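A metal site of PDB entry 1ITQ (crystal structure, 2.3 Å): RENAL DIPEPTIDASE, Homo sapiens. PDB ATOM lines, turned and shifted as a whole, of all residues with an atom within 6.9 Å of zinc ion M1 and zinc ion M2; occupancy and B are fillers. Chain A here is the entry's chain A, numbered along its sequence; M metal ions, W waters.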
ATOM      1  N   HIS A  20      -1.533   9.421   5.600  1.00  0.00           N
ATOM      2  CA  HIS A  20      -0.526   9.888   4.650  1.00  0.00           C
ATOM      3  C   HIS A  20       0.127  11.243   4.954  1.00  0.00           C
ATOM      4  O   HIS A  20      -0.463  12.291   4.732  1.00  0.00           O
ATOM      5  CB  HIS A  20      -1.131   9.930   3.257  1.00  0.00           C
ATOM      6  CG  HIS A  20      -0.128  10.118   2.164  1.00  0.00           C
ATOM      7  ND1 HIS A  20       0.561   9.079   1.575  1.00  0.00           N
ATOM      8  CD2 HIS A  20       0.307  11.245   1.550  1.00  0.00           C
ATOM      9  CE1 HIS A  20       1.361   9.610   0.642  1.00  0.00           C
ATOM     10  NE2 HIS A  20       1.242  10.919   0.600  1.00  0.00           N
ATOM     11  N   ASN A  21       1.379  11.210   5.411  1.00  0.00           N
ATOM     12  CA  ASN A  21       2.135  12.430   5.698  1.00  0.00           C
ATOM     13  C   ASN A  21       3.469  12.391   4.945  1.00  0.00           C
ATOM     14  O   ASN A  21       4.259  11.456   5.124  1.00  0.00           O
ATOM     15  CB  ASN A  21       2.378  12.607   7.188  1.00  0.00           C
ATOM     16  CG  ASN A  21       3.022  13.941   7.502  1.00  0.00           C
ATOM     17  OD1 ASN A  21       4.052  14.308   6.930  1.00  0.00           O
ATOM     18  ND2 ASN A  21       2.409  14.696   8.404  1.00  0.00           N
ATOM     19  N   ASP A  22       3.724  13.433   4.159  1.00  0.00           N
ATOM     20  CA  ASP A  22       4.923  13.506   3.357  1.00  0.00           C
ATOM     21  C   ASP A  22       6.101  14.244   3.941  1.00  0.00           C
ATOM     22  O   ASP A  22       6.832  14.917   3.209  1.00  0.00           O
ATOM     23  CB  ASP A  22       4.611  14.078   1.994  1.00  0.00           C
ATOM     24  CG  ASP A  22       3.918  13.082   1.110  1.00  0.00           C
ATOM     25  OD1 ASP A  22       2.710  13.268   0.857  1.00  0.00           O
ATOM     26  OD2 ASP A  22       4.583  12.116   0.678  1.00  0.00           O
ATOM     27  N   SER A  66       4.815   8.578   4.635  1.00  0.00           N
ATOM     28  CA  SER A  66       4.923   8.322   3.223  1.00  0.00           C
ATOM     29  C   SER A  66       6.348   8.263   2.695  1.00  0.00           C
ATOM     30  O   SER A  66       7.097   9.227   2.795  1.00  0.00           O
ATOM     31  CB  SER A  66       4.146   9.399   2.461  1.00  0.00           C
ATOM     32  OG  SER A  66       4.412   9.318   1.084  1.00  0.00           O
ATOM     33  N   TYR A  68       8.037   8.345  -0.346  1.00  0.00           N
ATOM     34  CA  TYR A  68       7.724   8.775  -1.687  1.00  0.00           C
ATOM     35  C   TYR A  68       8.905   9.215  -2.522  1.00  0.00           C
ATOM     36  O   TYR A  68       9.806   9.893  -2.040  1.00  0.00           O
ATOM     37  CB  TYR A  68       6.700   9.926  -1.576  1.00  0.00           C
ATOM     38  CG  TYR A  68       6.548  10.759  -2.819  1.00  0.00           C
ATOM     39  CD1 TYR A  68       7.137  12.011  -2.913  1.00  0.00           C
ATOM     40  CD2 TYR A  68       5.848  10.283  -3.924  1.00  0.00           C
ATOM     41  CE1 TYR A  68       7.040  12.771  -4.073  1.00  0.00           C
ATOM     42  CE2 TYR A  68       5.736  11.012  -5.081  1.00  0.00           C
ATOM     43  CZ  TYR A  68       6.332  12.256  -5.156  1.00  0.00           C
ATOM     44  OH  TYR A  68       6.226  12.973  -6.330  1.00  0.00           O
ATOM     45  N   GLU A 125       4.338   5.129  -1.485  1.00  0.00           N
ATOM     46  CA  GLU A 125       3.469   5.755  -2.457  1.00  0.00           C
ATOM     47  C   GLU A 125       3.889   5.698  -3.914  1.00  0.00           C
ATOM     48  O   GLU A 125       4.578   6.598  -4.412  1.00  0.00           O
ATOM     49  CB  GLU A 125       3.206   7.207  -2.062  1.00  0.00           C
ATOM     50  CG  GLU A 125       2.242   7.882  -2.985  1.00  0.00           C
ATOM     51  CD  GLU A 125       1.998   9.310  -2.601  1.00  0.00           C
ATOM     52  OE1 GLU A 125       2.930   9.966  -2.103  1.00  0.00           O
ATOM     53  OE2 GLU A 125       0.863   9.769  -2.810  1.00  0.00           O
ATOM     54  N   TYR A 147       1.766  -0.542   3.366  1.00  0.00           N
ATOM     55  CA  TYR A 147       0.752  -0.154   2.395  1.00  0.00           C
ATOM     56  C   TYR A 147       1.490   0.292   1.167  1.00  0.00           C
ATOM     57  O   TYR A 147       2.614   0.777   1.266  1.00  0.00           O
ATOM     58  CB  TYR A 147      -0.305   0.852   2.931  1.00  0.00           C
ATOM     59  CG  TYR A 147      -0.076   2.361   2.862  1.00  0.00           C
ATOM     60  CD1 TYR A 147       0.333   3.005   1.701  1.00  0.00           C
ATOM     61  CD2 TYR A 147      -0.365   3.155   3.978  1.00  0.00           C
ATOM     62  CE1 TYR A 147       0.451   4.411   1.647  1.00  0.00           C
ATOM     63  CE2 TYR A 147      -0.245   4.547   3.928  1.00  0.00           C
ATOM     64  CZ  TYR A 147       0.153   5.166   2.785  1.00  0.00           C
ATOM     65  OH  TYR A 147       0.257   6.549   2.764  1.00  0.00           O
ATOM     66  N   THR A 149       0.739   2.259  -2.415  1.00  0.00           N
ATOM     67  CA  THR A 149      -0.180   3.004  -3.243  1.00  0.00           C
ATOM     68  C   THR A 149       0.174   2.458  -4.624  1.00  0.00           C
ATOM     69  O   THR A 149       1.245   2.781  -5.157  1.00  0.00           O
ATOM     70  CB  THR A 149       0.118   4.510  -3.174  1.00  0.00           C
ATOM     71  OG1 THR A 149       0.204   4.915  -1.808  1.00  0.00           O
ATOM     72  CG2 THR A 149      -0.978   5.298  -3.839  1.00  0.00           C
ATOM     73  N   HIS A 152       1.109   6.362  -8.477  1.00  0.00           N
ATOM     74  CA  HIS A 152       1.157   7.732  -8.046  1.00  0.00           C
ATOM     75  C   HIS A 152       0.553   8.474  -9.225  1.00  0.00           C
ATOM     76  O   HIS A 152      -0.426   8.012  -9.803  1.00  0.00           O
ATOM     77  CB  HIS A 152       2.593   8.173  -7.785  1.00  0.00           C
ATOM     78  CG  HIS A 152       2.668   9.482  -7.094  1.00  0.00           C
ATOM     79  ND1 HIS A 152       2.990  10.652  -7.747  1.00  0.00           N
ATOM     80  CD2 HIS A 152       2.398   9.824  -5.809  1.00  0.00           C
ATOM     81  CE1 HIS A 152       2.911  11.657  -6.896  1.00  0.00           C
ATOM     82  NE2 HIS A 152       2.549  11.186  -5.719  1.00  0.00           N
ATOM     83  N   SER A 153       1.126   9.604  -9.605  1.00  0.00           N
ATOM     84  CA  SER A 153       0.571  10.345 -10.730  1.00  0.00           C
ATOM     85  C   SER A 153       1.146   9.891 -12.057  1.00  0.00           C
ATOM     86  O   SER A 153       1.456  10.713 -12.930  1.00  0.00           O
ATOM     87  CB  SER A 153       0.741  11.846 -10.532  1.00  0.00           C
ATOM     88  OG  SER A 153      -0.115  12.308  -9.501  1.00  0.00           O
ATOM     89  N   ALA A 197      -5.305   5.279  -3.456  1.00  0.00           N
ATOM     90  CA  ALA A 197      -5.183   6.704  -3.697  1.00  0.00           C
ATOM     91  C   ALA A 197      -4.351   6.827  -4.972  1.00  0.00           C
ATOM     92  O   ALA A 197      -3.486   5.995  -5.223  1.00  0.00           O
ATOM     93  CB  ALA A 197      -4.479   7.366  -2.540  1.00  0.00           C
ATOM     94  N   HIS A 198      -4.672   7.807  -5.802  1.00  0.00           N
ATOM     95  CA  HIS A 198      -3.948   8.022  -7.050  1.00  0.00           C
ATOM     96  C   HIS A 198      -4.247   7.116  -8.253  1.00  0.00           C
ATOM     97  O   HIS A 198      -3.789   7.426  -9.358  1.00  0.00           O
ATOM     98  CB  HIS A 198      -2.445   8.008  -6.802  1.00  0.00           C
ATOM     99  CG  HIS A 198      -1.912   9.282  -6.224  1.00  0.00           C
ATOM    100  ND1 HIS A 198      -1.592  10.390  -6.985  1.00  0.00           N
ATOM    101  CD2 HIS A 198      -1.571   9.588  -4.959  1.00  0.00           C
ATOM    102  CE1 HIS A 198      -1.058  11.306  -6.161  1.00  0.00           C
ATOM    103  NE2 HIS A 198      -1.034  10.868  -4.916  1.00  0.00           N
ATOM    104  N   SER A 218      -5.568   5.998   1.170  1.00  0.00           N
ATOM    105  CA  SER A 218      -4.812   6.664   2.244  1.00  0.00           C
ATOM    106  C   SER A 218      -4.956   8.179   2.308  1.00  0.00           C
ATOM    107  O   SER A 218      -4.678   8.772   3.334  1.00  0.00           O
ATOM    108  CB  SER A 218      -3.340   6.288   2.156  1.00  0.00           C
ATOM    109  OG  SER A 218      -2.793   6.764   0.952  1.00  0.00           O
ATOM    110  N   HIS A 219      -5.284   8.788   1.175  1.00  0.00           N
ATOM    111  CA  HIS A 219      -5.484  10.223   1.113  1.00  0.00           C
ATOM    112  C   HIS A 219      -6.356  10.627  -0.084  1.00  0.00           C
ATOM    113  O   HIS A 219      -5.889  11.267  -1.028  1.00  0.00           O
ATOM    114  CB  HIS A 219      -4.158  11.018   1.179  1.00  0.00           C
ATOM    115  CG  HIS A 219      -3.138  10.596   0.174  1.00  0.00           C
ATOM    116  ND1 HIS A 219      -2.524   9.362   0.162  1.00  0.00           N
ATOM    117  CD2 HIS A 219      -2.569  11.294  -0.836  1.00  0.00           C
ATOM    118  CE1 HIS A 219      -1.629   9.349  -0.820  1.00  0.00           C
ATOM    119  NE2 HIS A 219      -1.612  10.504  -1.460  1.00  0.00           N
ATOM    120  N   ARG A 230      -8.905  12.682  -8.313  1.00  0.00           N
ATOM    121  CA  ARG A 230      -8.104  12.221  -7.207  1.00  0.00           C
ATOM    122  C   ARG A 230      -9.085  11.859  -6.108  1.00  0.00           C
ATOM    123  O   ARG A 230      -8.702  11.431  -5.036  1.00  0.00           O
ATOM    124  CB  ARG A 230      -7.154  13.318  -6.727  1.00  0.00           C
ATOM    125  CG  ARG A 230      -5.759  13.186  -7.292  1.00  0.00           C
ATOM    126  CD  ARG A 230      -5.127  11.879  -6.806  1.00  0.00           C
ATOM    127  NE  ARG A 230      -4.596  11.996  -5.447  1.00  0.00           N
ATOM    128  CZ  ARG A 230      -5.034  11.318  -4.392  1.00  0.00           C
ATOM    129  NH1 ARG A 230      -4.466  11.498  -3.214  1.00  0.00           N
ATOM    130  NH2 ARG A 230      -6.058  10.478  -4.497  1.00  0.00           N
ATOM    131  N   ASN A 250      -8.345  13.466   2.339  1.00  0.00           N
ATOM    132  CA  ASN A 250      -7.249  14.354   1.980  1.00  0.00           C
ATOM    133  C   ASN A 250      -7.681  15.809   2.221  1.00  0.00           C
ATOM    134  O   ASN A 250      -8.734  16.237   1.725  1.00  0.00           O
ATOM    135  CB  ASN A 250      -6.930  14.151   0.491  1.00  0.00           C
ATOM    136  CG  ASN A 250      -5.644  14.796   0.064  1.00  0.00           C
ATOM    137  OD1 ASN A 250      -5.286  15.869   0.531  1.00  0.00           O
ATOM    138  ND2 ASN A 250      -4.928  14.149  -0.864  1.00  0.00           N
ATOM    139  N   TYR A 255      -8.892  19.622  -3.507  1.00  0.00           N
ATOM    140  CA  TYR A 255      -9.617  18.361  -3.568  1.00  0.00           C
ATOM    141  C   TYR A 255     -10.817  18.485  -2.626  1.00  0.00           C
ATOM    142  O   TYR A 255     -11.750  17.670  -2.655  1.00  0.00           O
ATOM    143  CB  TYR A 255      -8.743  17.192  -3.103  1.00  0.00           C
ATOM    144  CG  TYR A 255      -7.560  16.872  -3.999  1.00  0.00           C
ATOM    145  CD1 TYR A 255      -7.402  17.470  -5.250  1.00  0.00           C
ATOM    146  CD2 TYR A 255      -6.576  15.991  -3.558  1.00  0.00           C
ATOM    147  CE1 TYR A 255      -6.300  17.195  -6.038  1.00  0.00           C
ATOM    148  CE2 TYR A 255      -5.458  15.701  -4.353  1.00  0.00           C
ATOM    149  CZ  TYR A 255      -5.321  16.312  -5.576  1.00  0.00           C
ATOM    150  OH  TYR A 255      -4.200  16.039  -6.313  1.00  0.00           O
ATOM    151  N   ASP A 288      -2.595  14.381   4.112  1.00  0.00           N
ATOM    152  CA  ASP A 288      -1.666  14.754   3.048  1.00  0.00           C
ATOM    153  C   ASP A 288      -0.814  15.962   3.460  1.00  0.00           C
ATOM    154  O   ASP A 288      -0.347  16.736   2.619  1.00  0.00           O
ATOM    155  CB  ASP A 288      -2.407  15.032   1.726  1.00  0.00           C
ATOM    156  CG  ASP A 288      -1.536  14.806   0.508  1.00  0.00           C
ATOM    157  OD1 ASP A 288      -0.357  14.416   0.661  1.00  0.00           O
ATOM    158  OD2 ASP A 288      -2.033  15.026  -0.622  1.00  0.00           O
ATOM    159  N   ASP A 290       2.293  18.133   4.440  1.00  0.00           N
ATOM    160  CA  ASP A 290       3.673  18.168   3.972  1.00  0.00           C
ATOM    161  C   ASP A 290       3.858  17.598   2.574  1.00  0.00           C
ATOM    162  O   ASP A 290       4.968  17.510   2.061  1.00  0.00           O
ATOM    163  CB  ASP A 290       4.616  17.532   4.985  1.00  0.00           C
ATOM    164  CG  ASP A 290       5.031  18.496   6.064  1.00  0.00           C
ATOM    165  OD1 ASP A 290       5.292  19.668   5.719  1.00  0.00           O
ATOM    166  OD2 ASP A 290       5.092  18.112   7.253  1.00  0.00           O
ATOM    167  N   GLY A 291       2.738  17.264   1.957  1.00  0.00           N
ATOM    168  CA  GLY A 291       2.774  16.751   0.605  1.00  0.00           C
ATOM    169  C   GLY A 291       2.127  17.757  -0.320  1.00  0.00           C
ATOM    170  O   GLY A 291       2.435  17.803  -1.510  1.00  0.00           O
ATOM    171  N   VAL A 292       1.223  18.573   0.245  1.00  0.00           N
ATOM    172  CA  VAL A 292       0.494  19.599  -0.504  1.00  0.00           C
ATOM    173  C   VAL A 292       0.855  21.016  -0.056  1.00  0.00           C
ATOM    174  O   VAL A 292       1.188  21.233   1.108  1.00  0.00           O
ATOM    175  CB  VAL A 292      -1.030  19.377  -0.392  1.00  0.00           C
ATOM    176  CG1 VAL A 292      -1.422  18.117  -1.150  1.00  0.00           C
ATOM    177  CG2 VAL A 292      -1.451  19.265   1.071  1.00  0.00           C
HETATM  178 ZN    ZN M   1      -0.500  11.564  -2.829  1.00  0.00          ZN
HETATM  179 ZN    ZN M   2       2.244  11.883  -0.878  1.00  0.00          ZN
HETATM  180  O   HOH W   1      -1.900  13.705  -3.468  1.00  0.00           O
HETATM  181  O   HOH W   2       0.908  13.910  -2.231  1.00  0.00           O
HETATM  182  O   HOH W   3       3.588  12.751  -2.429  1.00  0.00           O
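A ring nitrogen (ND1) of His 20 lies close to a ring nitrogen (ND1) of His 219, 3.4 Å away.
N of Asp 288 is in hydrogen-bond range of O of His 20 (3.0 Å).
ND1 of His 20 lies within hydrogen-bond range of OH of Tyr 147, at 2.8 Å.
O of His 219 is in hydrogen-bond range of NH1 of Arg 230, 2.6 Å away.
A ring nitrogen (ND1) of His 219 is in hydrogen-bond range of the side-chain hydroxyl of Ser 218 (2.7 Å).
A ring nitrogen (ND1) of His 198 sits at hydrogen-bond distance from the side-chain hydroxyl (OG) of Ser 153.
OD2 of Asp 22 lies within hydrogen-bond range of OG of Ser 66 (2.8 Å).
The side-chain carboxylate of Asp 288 is in hydrogen-bond range of the side-chain amide nitrogen of Asn 250.
Residues that only touch zinc ion M1: Arg 230 (3.99 Å).
Ser 66 touches zinc ion M2.
OD1 of Asp 288 touches zinc ion M2, at 3.9 Å.
Of the 21 residues printed, 5 come within 4 Å of zinc ion M2.
The nearest printed residue that does not touch zinc ion M2 is His 219 (4.1 Å).
Zinc ion M1 is bound by a ring nitrogen (NE2) of His 219 (2.1 Å), the side-chain carboxylate of Glu 125 (2.3 Å) and a ring nitrogen (NE2) of His 198 (2.3 Å).
Zinc ion M1 has three donor atoms within binding distance.
Slightly farther from zinc ion M1 lies water W1 (2.6 Å).
Slightly farther from zinc ion M1 lies water W2 (2.8 Å).
Zinc ion M2 is bound by a ring nitrogen (NE2) of His 20 (2.0 Å), water W3 (2.2 Å), the side-chain carboxylate of Asp 22 (2.3 Å) and the side-chain carboxylate of Glu 125 (2.4 Å).
Slightly farther from zinc ion M2 lies water W2 (2.8 Å).
Slightly farther from zinc ion M2 lies the side-chain carboxylate (OD2) of Asp 22 (2.8 Å).
Water W1 bridges the side-chain carboxylate (OD2) of Asp 288 (3.1 Å) and the guanidinium group (NH1) of Arg 230 (3.4 Å).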
